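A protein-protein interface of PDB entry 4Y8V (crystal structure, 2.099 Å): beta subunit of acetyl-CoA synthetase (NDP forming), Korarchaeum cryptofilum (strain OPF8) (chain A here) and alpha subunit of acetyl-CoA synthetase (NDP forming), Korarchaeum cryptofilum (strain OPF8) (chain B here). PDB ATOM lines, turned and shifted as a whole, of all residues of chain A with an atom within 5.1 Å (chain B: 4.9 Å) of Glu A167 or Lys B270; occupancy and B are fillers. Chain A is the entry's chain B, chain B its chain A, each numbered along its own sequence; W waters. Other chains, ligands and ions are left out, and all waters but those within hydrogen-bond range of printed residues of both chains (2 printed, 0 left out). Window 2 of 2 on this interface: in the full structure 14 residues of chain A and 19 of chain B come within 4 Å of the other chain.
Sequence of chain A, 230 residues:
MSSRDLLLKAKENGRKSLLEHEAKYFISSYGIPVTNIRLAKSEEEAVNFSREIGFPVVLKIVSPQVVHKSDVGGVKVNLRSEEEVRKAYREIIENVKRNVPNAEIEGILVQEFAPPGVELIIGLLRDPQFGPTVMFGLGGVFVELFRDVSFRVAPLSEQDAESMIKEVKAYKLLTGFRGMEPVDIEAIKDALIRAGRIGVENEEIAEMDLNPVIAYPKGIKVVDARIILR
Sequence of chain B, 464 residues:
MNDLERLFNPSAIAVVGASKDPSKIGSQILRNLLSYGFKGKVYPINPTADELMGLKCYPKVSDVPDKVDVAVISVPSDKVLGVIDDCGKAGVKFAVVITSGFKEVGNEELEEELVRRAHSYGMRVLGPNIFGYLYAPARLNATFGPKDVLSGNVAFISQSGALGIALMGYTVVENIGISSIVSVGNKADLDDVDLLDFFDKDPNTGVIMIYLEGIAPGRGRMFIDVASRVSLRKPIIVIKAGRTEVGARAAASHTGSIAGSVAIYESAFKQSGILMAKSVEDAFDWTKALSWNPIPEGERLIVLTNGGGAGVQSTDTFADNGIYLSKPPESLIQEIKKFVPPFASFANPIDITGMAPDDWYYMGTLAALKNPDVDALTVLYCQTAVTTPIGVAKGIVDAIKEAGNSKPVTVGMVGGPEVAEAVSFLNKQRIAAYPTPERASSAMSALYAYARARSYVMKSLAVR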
ATOM      1  N   VAL A 149      -2.592  -9.579 -25.358  1.00  0.00           N
ATOM      2  CA  VAL A 149      -2.428 -10.955 -24.889  1.00  0.00           C
ATOM      3  C   VAL A 149      -3.460 -11.330 -23.832  1.00  0.00           C
ATOM      4  O   VAL A 149      -3.921 -10.472 -23.082  1.00  0.00           O
ATOM      5  CB  VAL A 149      -1.031 -11.174 -24.280  1.00  0.00           C
ATOM      6  CG1 VAL A 149       0.044 -11.068 -25.346  1.00  0.00           C
ATOM      7  CG2 VAL A 149      -0.779 -10.169 -23.164  1.00  0.00           C
ATOM      8  N   SER A 150      -3.799 -12.614 -23.761  1.00  0.00           N
ATOM      9  CA  SER A 150      -4.630 -13.138 -22.680  1.00  0.00           C
ATOM     10  C   SER A 150      -3.844 -14.152 -21.847  1.00  0.00           C
ATOM     11  O   SER A 150      -2.858 -14.725 -22.317  1.00  0.00           O
ATOM     12  CB  SER A 150      -5.902 -13.782 -23.232  1.00  0.00           C
ATOM     13  OG  SER A 150      -5.601 -14.818 -24.149  1.00  0.00           O
ATOM     14  N   PHE A 151      -4.293 -14.354 -20.611  1.00  0.00           N
ATOM     15  CA  PHE A 151      -3.650 -15.268 -19.670  1.00  0.00           C
ATOM     16  C   PHE A 151      -4.667 -16.189 -19.017  1.00  0.00           C
ATOM     17  O   PHE A 151      -5.795 -15.772 -18.737  1.00  0.00           O
ATOM     18  CB  PHE A 151      -2.914 -14.505 -18.566  1.00  0.00           C
ATOM     19  CG  PHE A 151      -1.865 -13.554 -19.063  1.00  0.00           C
ATOM     20  CD1 PHE A 151      -2.202 -12.261 -19.424  1.00  0.00           C
ATOM     21  CD2 PHE A 151      -0.536 -13.945 -19.136  1.00  0.00           C
ATOM     22  CE1 PHE A 151      -1.238 -11.377 -19.871  1.00  0.00           C
ATOM     23  CE2 PHE A 151       0.437 -13.066 -19.582  1.00  0.00           C
ATOM     24  CZ  PHE A 151       0.087 -11.780 -19.950  1.00  0.00           C
ATOM     25  N   ARG A 152      -4.267 -17.440 -18.798  1.00  0.00           N
ATOM     26  CA  ARG A 152      -5.007 -18.354 -17.930  1.00  0.00           C
ATOM     27  C   ARG A 152      -4.034 -19.158 -17.072  1.00  0.00           C
ATOM     28  O   ARG A 152      -3.001 -19.620 -17.558  1.00  0.00           O
ATOM     29  CB  ARG A 152      -5.891 -19.302 -18.742  1.00  0.00           C
ATOM     30  CG  ARG A 152      -7.048 -18.636 -19.471  1.00  0.00           C
ATOM     31  CD  ARG A 152      -8.100 -18.094 -18.510  1.00  0.00           C
ATOM     32  NE  ARG A 152      -9.282 -17.625 -19.227  1.00  0.00           N
ATOM     33  CZ  ARG A 152      -9.365 -16.463 -19.867  1.00  0.00           C
ATOM     34  NH1 ARG A 152      -8.331 -15.632 -19.888  1.00  0.00           N
ATOM     35  NH2 ARG A 152     -10.484 -16.132 -20.494  1.00  0.00           N
ATOM     36  N   SER A 163     -12.197 -19.381 -24.067  1.00  0.00           N
ATOM     37  CA  SER A 163     -12.513 -18.014 -23.670  1.00  0.00           C
ATOM     38  C   SER A 163     -11.293 -17.107 -23.820  1.00  0.00           C
ATOM     39  O   SER A 163     -11.428 -15.949 -24.213  1.00  0.00           O
ATOM     40  CB  SER A 163     -13.029 -17.967 -22.228  1.00  0.00           C
ATOM     41  OG  SER A 163     -12.021 -18.329 -21.300  1.00  0.00           O
ATOM     42  N   MET A 164     -10.101 -17.625 -23.531  1.00  0.00           N
ATOM     43  CA  MET A 164      -8.916 -16.773 -23.605  1.00  0.00           C
ATOM     44  C   MET A 164      -8.620 -16.438 -25.068  1.00  0.00           C
ATOM     45  O   MET A 164      -8.196 -15.324 -25.370  1.00  0.00           O
ATOM     46  CB  MET A 164      -7.705 -17.434 -22.927  1.00  0.00           C
ATOM     47  CG  MET A 164      -6.941 -18.448 -23.763  1.00  0.00           C
ATOM     48  SD  MET A 164      -5.682 -19.319 -22.805  1.00  0.00           S
ATOM     49  CE  MET A 164      -4.492 -18.009 -22.521  1.00  0.00           C
ATOM     50  N   ILE A 165      -8.927 -17.353 -25.985  1.00  0.00           N
ATOM     51  CA  ILE A 165      -8.762 -17.045 -27.408  1.00  0.00           C
ATOM     52  C   ILE A 165      -9.722 -15.936 -27.835  1.00  0.00           C
ATOM     53  O   ILE A 165      -9.313 -14.985 -28.498  1.00  0.00           O
ATOM     54  CB  ILE A 165      -8.989 -18.279 -28.306  1.00  0.00           C
ATOM     55  CG1 ILE A 165      -7.889 -19.314 -28.069  1.00  0.00           C
ATOM     56  CG2 ILE A 165      -8.991 -17.879 -29.790  1.00  0.00           C
ATOM     57  CD1 ILE A 165      -8.185 -20.678 -28.660  1.00  0.00           C
ATOM     58  N   LYS A 166     -10.991 -16.054 -27.462  1.00  0.00           N
ATOM     59  CA  LYS A 166     -11.986 -15.051 -27.844  1.00  0.00           C
ATOM     60  C   LYS A 166     -11.746 -13.708 -27.160  1.00  0.00           C
ATOM     61  O   LYS A 166     -12.301 -12.686 -27.565  1.00  0.00           O
ATOM     62  CB  LYS A 166     -13.392 -15.555 -27.524  1.00  0.00           C
ATOM     63  CG  LYS A 166     -13.795 -16.747 -28.365  1.00  0.00           C
ATOM     64  CD  LYS A 166     -15.157 -17.277 -27.981  1.00  0.00           C
ATOM     65  CE  LYS A 166     -15.653 -18.273 -29.011  1.00  0.00           C
ATOM     66  NZ  LYS A 166     -16.494 -19.333 -28.398  1.00  0.00           N
ATOM     67  N   GLU A 167     -10.890 -13.706 -26.144  1.00  0.00           N
ATOM     68  CA  GLU A 167     -10.695 -12.530 -25.307  1.00  0.00           C
ATOM     69  C   GLU A 167      -9.807 -11.469 -25.960  1.00  0.00           C
ATOM     70  O   GLU A 167      -9.999 -10.276 -25.735  1.00  0.00           O
ATOM     71  CB  GLU A 167     -10.101 -12.961 -23.964  1.00  0.00           C
ATOM     72  CG  GLU A 167      -9.746 -11.824 -23.023  1.00  0.00           C
ATOM     73  CD  GLU A 167      -9.128 -12.325 -21.734  1.00  0.00           C
ATOM     74  OE1 GLU A 167      -8.178 -11.678 -21.240  1.00  0.00           O
ATOM     75  OE2 GLU A 167      -9.585 -13.367 -21.218  1.00  0.00           O
ATOM     76  N   VAL A 168      -8.834 -11.895 -26.758  1.00  0.00           N
ATOM     77  CA  VAL A 168      -7.863 -10.951 -27.306  1.00  0.00           C
ATOM     78  C   VAL A 168      -8.499 -10.043 -28.358  1.00  0.00           C
ATOM     79  O   VAL A 168      -9.368 -10.465 -29.120  1.00  0.00           O
ATOM     80  CB  VAL A 168      -6.649 -11.673 -27.933  1.00  0.00           C
ATOM     81  CG1 VAL A 168      -5.937 -12.518 -26.885  1.00  0.00           C
ATOM     82  CG2 VAL A 168      -7.070 -12.535 -29.121  1.00  0.00           C
ATOM     83  N   LYS A 169      -8.027  -8.802 -28.409  1.00  0.00           N
ATOM     84  CA  LYS A 169      -8.578  -7.795 -29.307  1.00  0.00           C
ATOM     85  C   LYS A 169      -8.434  -8.137 -30.791  1.00  0.00           C
ATOM     86  O   LYS A 169      -9.197  -7.633 -31.615  1.00  0.00           O
ATOM     87  CB  LYS A 169      -7.931  -6.437 -29.017  1.00  0.00           C
ATOM     88  CG  LYS A 169      -8.384  -5.843 -27.690  1.00  0.00           C
ATOM     89  CD  LYS A 169      -7.423  -4.806 -27.142  1.00  0.00           C
ATOM     90  CE  LYS A 169      -7.660  -4.602 -25.655  1.00  0.00           C
ATOM     91  NZ  LYS A 169      -6.677  -3.677 -25.033  1.00  0.00           N
ATOM     92  N   GLU B 266      -6.398 -10.724 -12.698  1.00  0.00           N
ATOM     93  CA  GLU B 266      -7.704 -10.601 -13.332  1.00  0.00           C
ATOM     94  C   GLU B 266      -8.170 -11.962 -13.839  1.00  0.00           C
ATOM     95  O   GLU B 266      -9.320 -12.359 -13.648  1.00  0.00           O
ATOM     96  CB  GLU B 266      -7.668  -9.596 -14.492  1.00  0.00           C
ATOM     97  CG  GLU B 266      -7.639  -8.131 -14.059  1.00  0.00           C
ATOM     98  CD  GLU B 266      -7.955  -7.160 -15.181  1.00  0.00           C
ATOM     99  OE1 GLU B 266      -8.584  -7.567 -16.183  1.00  0.00           O
ATOM    100  OE2 GLU B 266      -7.589  -5.969 -15.047  1.00  0.00           O
ATOM    101  N   SER B 267      -7.255 -12.698 -14.458  1.00  0.00           N
ATOM    102  CA  SER B 267      -7.571 -14.023 -14.976  1.00  0.00           C
ATOM    103  C   SER B 267      -7.866 -15.009 -13.851  1.00  0.00           C
ATOM    104  O   SER B 267      -8.777 -15.826 -13.964  1.00  0.00           O
ATOM    105  CB  SER B 267      -6.430 -14.534 -15.854  1.00  0.00           C
ATOM    106  OG  SER B 267      -6.328 -13.737 -17.021  1.00  0.00           O
ATOM    107  N   ALA B 268      -7.084 -14.946 -12.778  1.00  0.00           N
ATOM    108  CA  ALA B 268      -7.313 -15.798 -11.617  1.00  0.00           C
ATOM    109  C   ALA B 268      -8.704 -15.572 -11.026  1.00  0.00           C
ATOM    110  O   ALA B 268      -9.371 -16.516 -10.611  1.00  0.00           O
ATOM    111  CB  ALA B 268      -6.247 -15.562 -10.564  1.00  0.00           C
ATOM    112  N   PHE B 269      -9.130 -14.315 -10.951  1.00  0.00           N
ATOM    113  CA  PHE B 269     -10.451 -14.008 -10.409  1.00  0.00           C
ATOM    114  C   PHE B 269     -11.544 -14.536 -11.336  1.00  0.00           C
ATOM    115  O   PHE B 269     -12.563 -15.044 -10.870  1.00  0.00           O
ATOM    116  CB  PHE B 269     -10.615 -12.500 -10.190  1.00  0.00           C
ATOM    117  CG  PHE B 269      -9.713 -11.929  -9.121  1.00  0.00           C
ATOM    118  CD1 PHE B 269      -9.282 -12.703  -8.057  1.00  0.00           C
ATOM    119  CD2 PHE B 269      -9.307 -10.611  -9.183  1.00  0.00           C
ATOM    120  CE1 PHE B 269      -8.458 -12.169  -7.082  1.00  0.00           C
ATOM    121  CE2 PHE B 269      -8.486 -10.073  -8.215  1.00  0.00           C
ATOM    122  CZ  PHE B 269      -8.061 -10.851  -7.162  1.00  0.00           C
ATOM    123  N   LYS B 270     -11.332 -14.412 -12.642  1.00  0.00           N
ATOM    124  CA  LYS B 270     -12.269 -14.948 -13.625  1.00  0.00           C
ATOM    125  C   LYS B 270     -12.394 -16.467 -13.480  1.00  0.00           C
ATOM    126  O   LYS B 270     -13.493 -17.025 -13.493  1.00  0.00           O
ATOM    127  CB  LYS B 270     -11.825 -14.580 -15.046  1.00  0.00           C
ATOM    128  CG  LYS B 270     -12.739 -15.112 -16.150  1.00  0.00           C
ATOM    129  CD  LYS B 270     -12.190 -14.818 -17.542  1.00  0.00           C
ATOM    130  CE  LYS B 270     -12.306 -13.345 -17.912  1.00  0.00           C
ATOM    131  NZ  LYS B 270     -11.480 -13.006 -19.106  1.00  0.00           N
ATOM    132  N   GLN B 271     -11.261 -17.143 -13.324  1.00  0.00           N
ATOM    133  CA  GLN B 271     -11.272 -18.596 -13.170  1.00  0.00           C
ATOM    134  C   GLN B 271     -11.857 -18.984 -11.810  1.00  0.00           C
ATOM    135  O   GLN B 271     -12.311 -20.110 -11.609  1.00  0.00           O
ATOM    136  CB  GLN B 271      -9.859 -19.165 -13.341  1.00  0.00           C
ATOM    137  CG  GLN B 271      -9.305 -18.985 -14.750  1.00  0.00           C
ATOM    138  CD  GLN B 271      -7.846 -19.383 -14.875  1.00  0.00           C
ATOM    139  OE1 GLN B 271      -6.975 -18.528 -15.012  1.00  0.00           O
ATOM    140  NE2 GLN B 271      -7.577 -20.684 -14.846  1.00  0.00           N
ATOM    141  N   SER B 272     -11.875 -18.037 -10.878  1.00  0.00           N
ATOM    142  CA  SER B 272     -12.453 -18.273  -9.554  1.00  0.00           C
ATOM    143  C   SER B 272     -13.944 -17.938  -9.484  1.00  0.00           C
ATOM    144  O   SER B 272     -14.599 -18.224  -8.482  1.00  0.00           O
ATOM    145  CB  SER B 272     -11.702 -17.463  -8.499  1.00  0.00           C
ATOM    146  OG  SER B 272     -10.375 -17.934  -8.357  1.00  0.00           O
ATOM    147  N   GLY B 273     -14.476 -17.331 -10.540  1.00  0.00           N
ATOM    148  CA  GLY B 273     -15.863 -16.902 -10.555  1.00  0.00           C
ATOM    149  C   GLY B 273     -16.095 -15.664  -9.702  1.00  0.00           C
ATOM    150  O   GLY B 273     -17.234 -15.321  -9.383  1.00  0.00           O
ATOM    151  N   ILE B 274     -15.007 -14.972  -9.380  1.00  0.00           N
ATOM    152  CA  ILE B 274     -15.039 -13.805  -8.503  1.00  0.00           C
ATOM    153  C   ILE B 274     -15.430 -12.544  -9.266  1.00  0.00           C
ATOM    154  O   ILE B 274     -15.072 -12.389 -10.432  1.00  0.00           O
ATOM    155  CB  ILE B 274     -13.659 -13.597  -7.828  1.00  0.00           C
ATOM    156  CG1 ILE B 274     -13.453 -14.646  -6.733  1.00  0.00           C
ATOM    157  CG2 ILE B 274     -13.521 -12.181  -7.244  1.00  0.00           C
ATOM    158  CD1 ILE B 274     -12.037 -14.719  -6.196  1.00  0.00           C
ATOM    159  N   TYR B 456     -19.157 -19.958 -15.726  1.00  0.00           N
ATOM    160  CA  TYR B 456     -17.781 -20.095 -16.196  1.00  0.00           C
ATOM    161  C   TYR B 456     -17.098 -21.215 -15.424  1.00  0.00           C
ATOM    162  O   TYR B 456     -16.462 -22.093 -16.009  1.00  0.00           O
ATOM    163  CB  TYR B 456     -16.997 -18.787 -16.030  1.00  0.00           C
ATOM    164  CG  TYR B 456     -15.600 -18.840 -16.620  1.00  0.00           C
ATOM    165  CD1 TYR B 456     -14.575 -19.539 -15.988  1.00  0.00           C
ATOM    166  CD2 TYR B 456     -15.307 -18.192 -17.812  1.00  0.00           C
ATOM    167  CE1 TYR B 456     -13.301 -19.594 -16.533  1.00  0.00           C
ATOM    168  CE2 TYR B 456     -14.041 -18.239 -18.360  1.00  0.00           C
ATOM    169  CZ  TYR B 456     -13.042 -18.938 -17.721  1.00  0.00           C
ATOM    170  OH  TYR B 456     -11.791 -18.969 -18.294  1.00  0.00           O
ATOM    171  N   VAL B 457     -17.245 -21.180 -14.103  1.00  0.00           N
ATOM    172  CA  VAL B 457     -16.613 -22.168 -13.241  1.00  0.00           C
ATOM    173  C   VAL B 457     -17.151 -23.571 -13.523  1.00  0.00           C
ATOM    174  O   VAL B 457     -16.373 -24.520 -13.645  1.00  0.00           O
ATOM    175  CB  VAL B 457     -16.825 -21.819 -11.750  1.00  0.00           C
ATOM    176  CG1 VAL B 457     -16.393 -22.975 -10.843  1.00  0.00           C
ATOM    177  CG2 VAL B 457     -16.055 -20.554 -11.391  1.00  0.00           C
HETATM  178  O   HOH W   1     -13.090 -14.581 -21.121  1.00  0.00           O
HETATM  179  O   HOH W   2      -6.311 -12.900 -19.688  1.00  0.00           O
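Water W2 lies within hydrogen-bond range of the backbone NH (N) of Phe A151 (2.7 Å), the side-chain carboxylate (OE1) of Glu A167 (2.7 Å), the side-chain hydroxyl (OG) of Ser B267 (2.8 Å) and the guanidinium group (NH1) of Arg A152 (3.4 Å).
Water W1 bridges NZ of Lys B270 (3.0 Å) and NH2 of Arg A152 (3.1 Å).
Of the 11 printed residues of chain A, 4 touch a printed residue of chain B.
Hydrophobic or aromatic side chains of chain A within 4 Å of the printed part of chain B: Phe A151.
Of the 11 printed residues of chain B, 4 touch a printed residue of chain A.
Hydrophobic or aromatic side chains of chain B that line the printed part of chain A: Tyr B456.
Among the printed residues, 7 pairs touch across the chains.
Printed residues of chain B within 4 Å of Phe A151: Ser B267.
Printed residues of chain B within 4 Å of Arg A152: Ser B267 (3.98 Å), Lys B270 (3.6 Å), Gln B271 (3.5 Å) and Tyr B456 (3.0 Å).
Of the printed residues of chain B, Ser A163 touches Tyr B456 (3.1 Å).
Glu A167 touches just one residue of chain B: Lys B270.
Of chain A, only Arg A152 (3.6 Å) and Glu A167 (2.9 Å) come within 4 Å of Lys B270.
The nearest printed residue of chain B that does not touch Ser A163 is Lys B270 (5.1 Å).
The side-chain amino group of Lys B270 lies within salt-bridge range of the side-chain carboxylate of Glu A167, 2.9 Å away.
The side-chain hydroxyl of Tyr B456 lies within hydrogen-bond range of the side-chain hydroxyl of Ser A163, 3.1 Å away.
The backbone carbonyl oxygen of Phe A151 is in hydrogen-bond range of the side-chain hydroxyl of Ser B267 (2.7 Å).
The guanidinium group (NE) of Arg A152 lies within hydrogen-bond range of the side-chain hydroxyl (OH) of Tyr B456.
Among the printed residues, pairs that only touch across the chains: Arg A152 with Ser B267, Arg A152 with Lys B270 and Arg A152 with Gln B271.
NH1 of Arg A152 is in salt-bridge range of OE2 of Glu A167 (2.9 Å).
The side-chain hydroxyl of Ser A163 lies within hydrogen-bond range of the guanidinium group of Arg A152, 2.8 Å away.
The backbone carbonyl oxygen (O) of Ser B267 sits close to the side-chain amide oxygen (OE1) of Gln B271 (3.4 Å).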
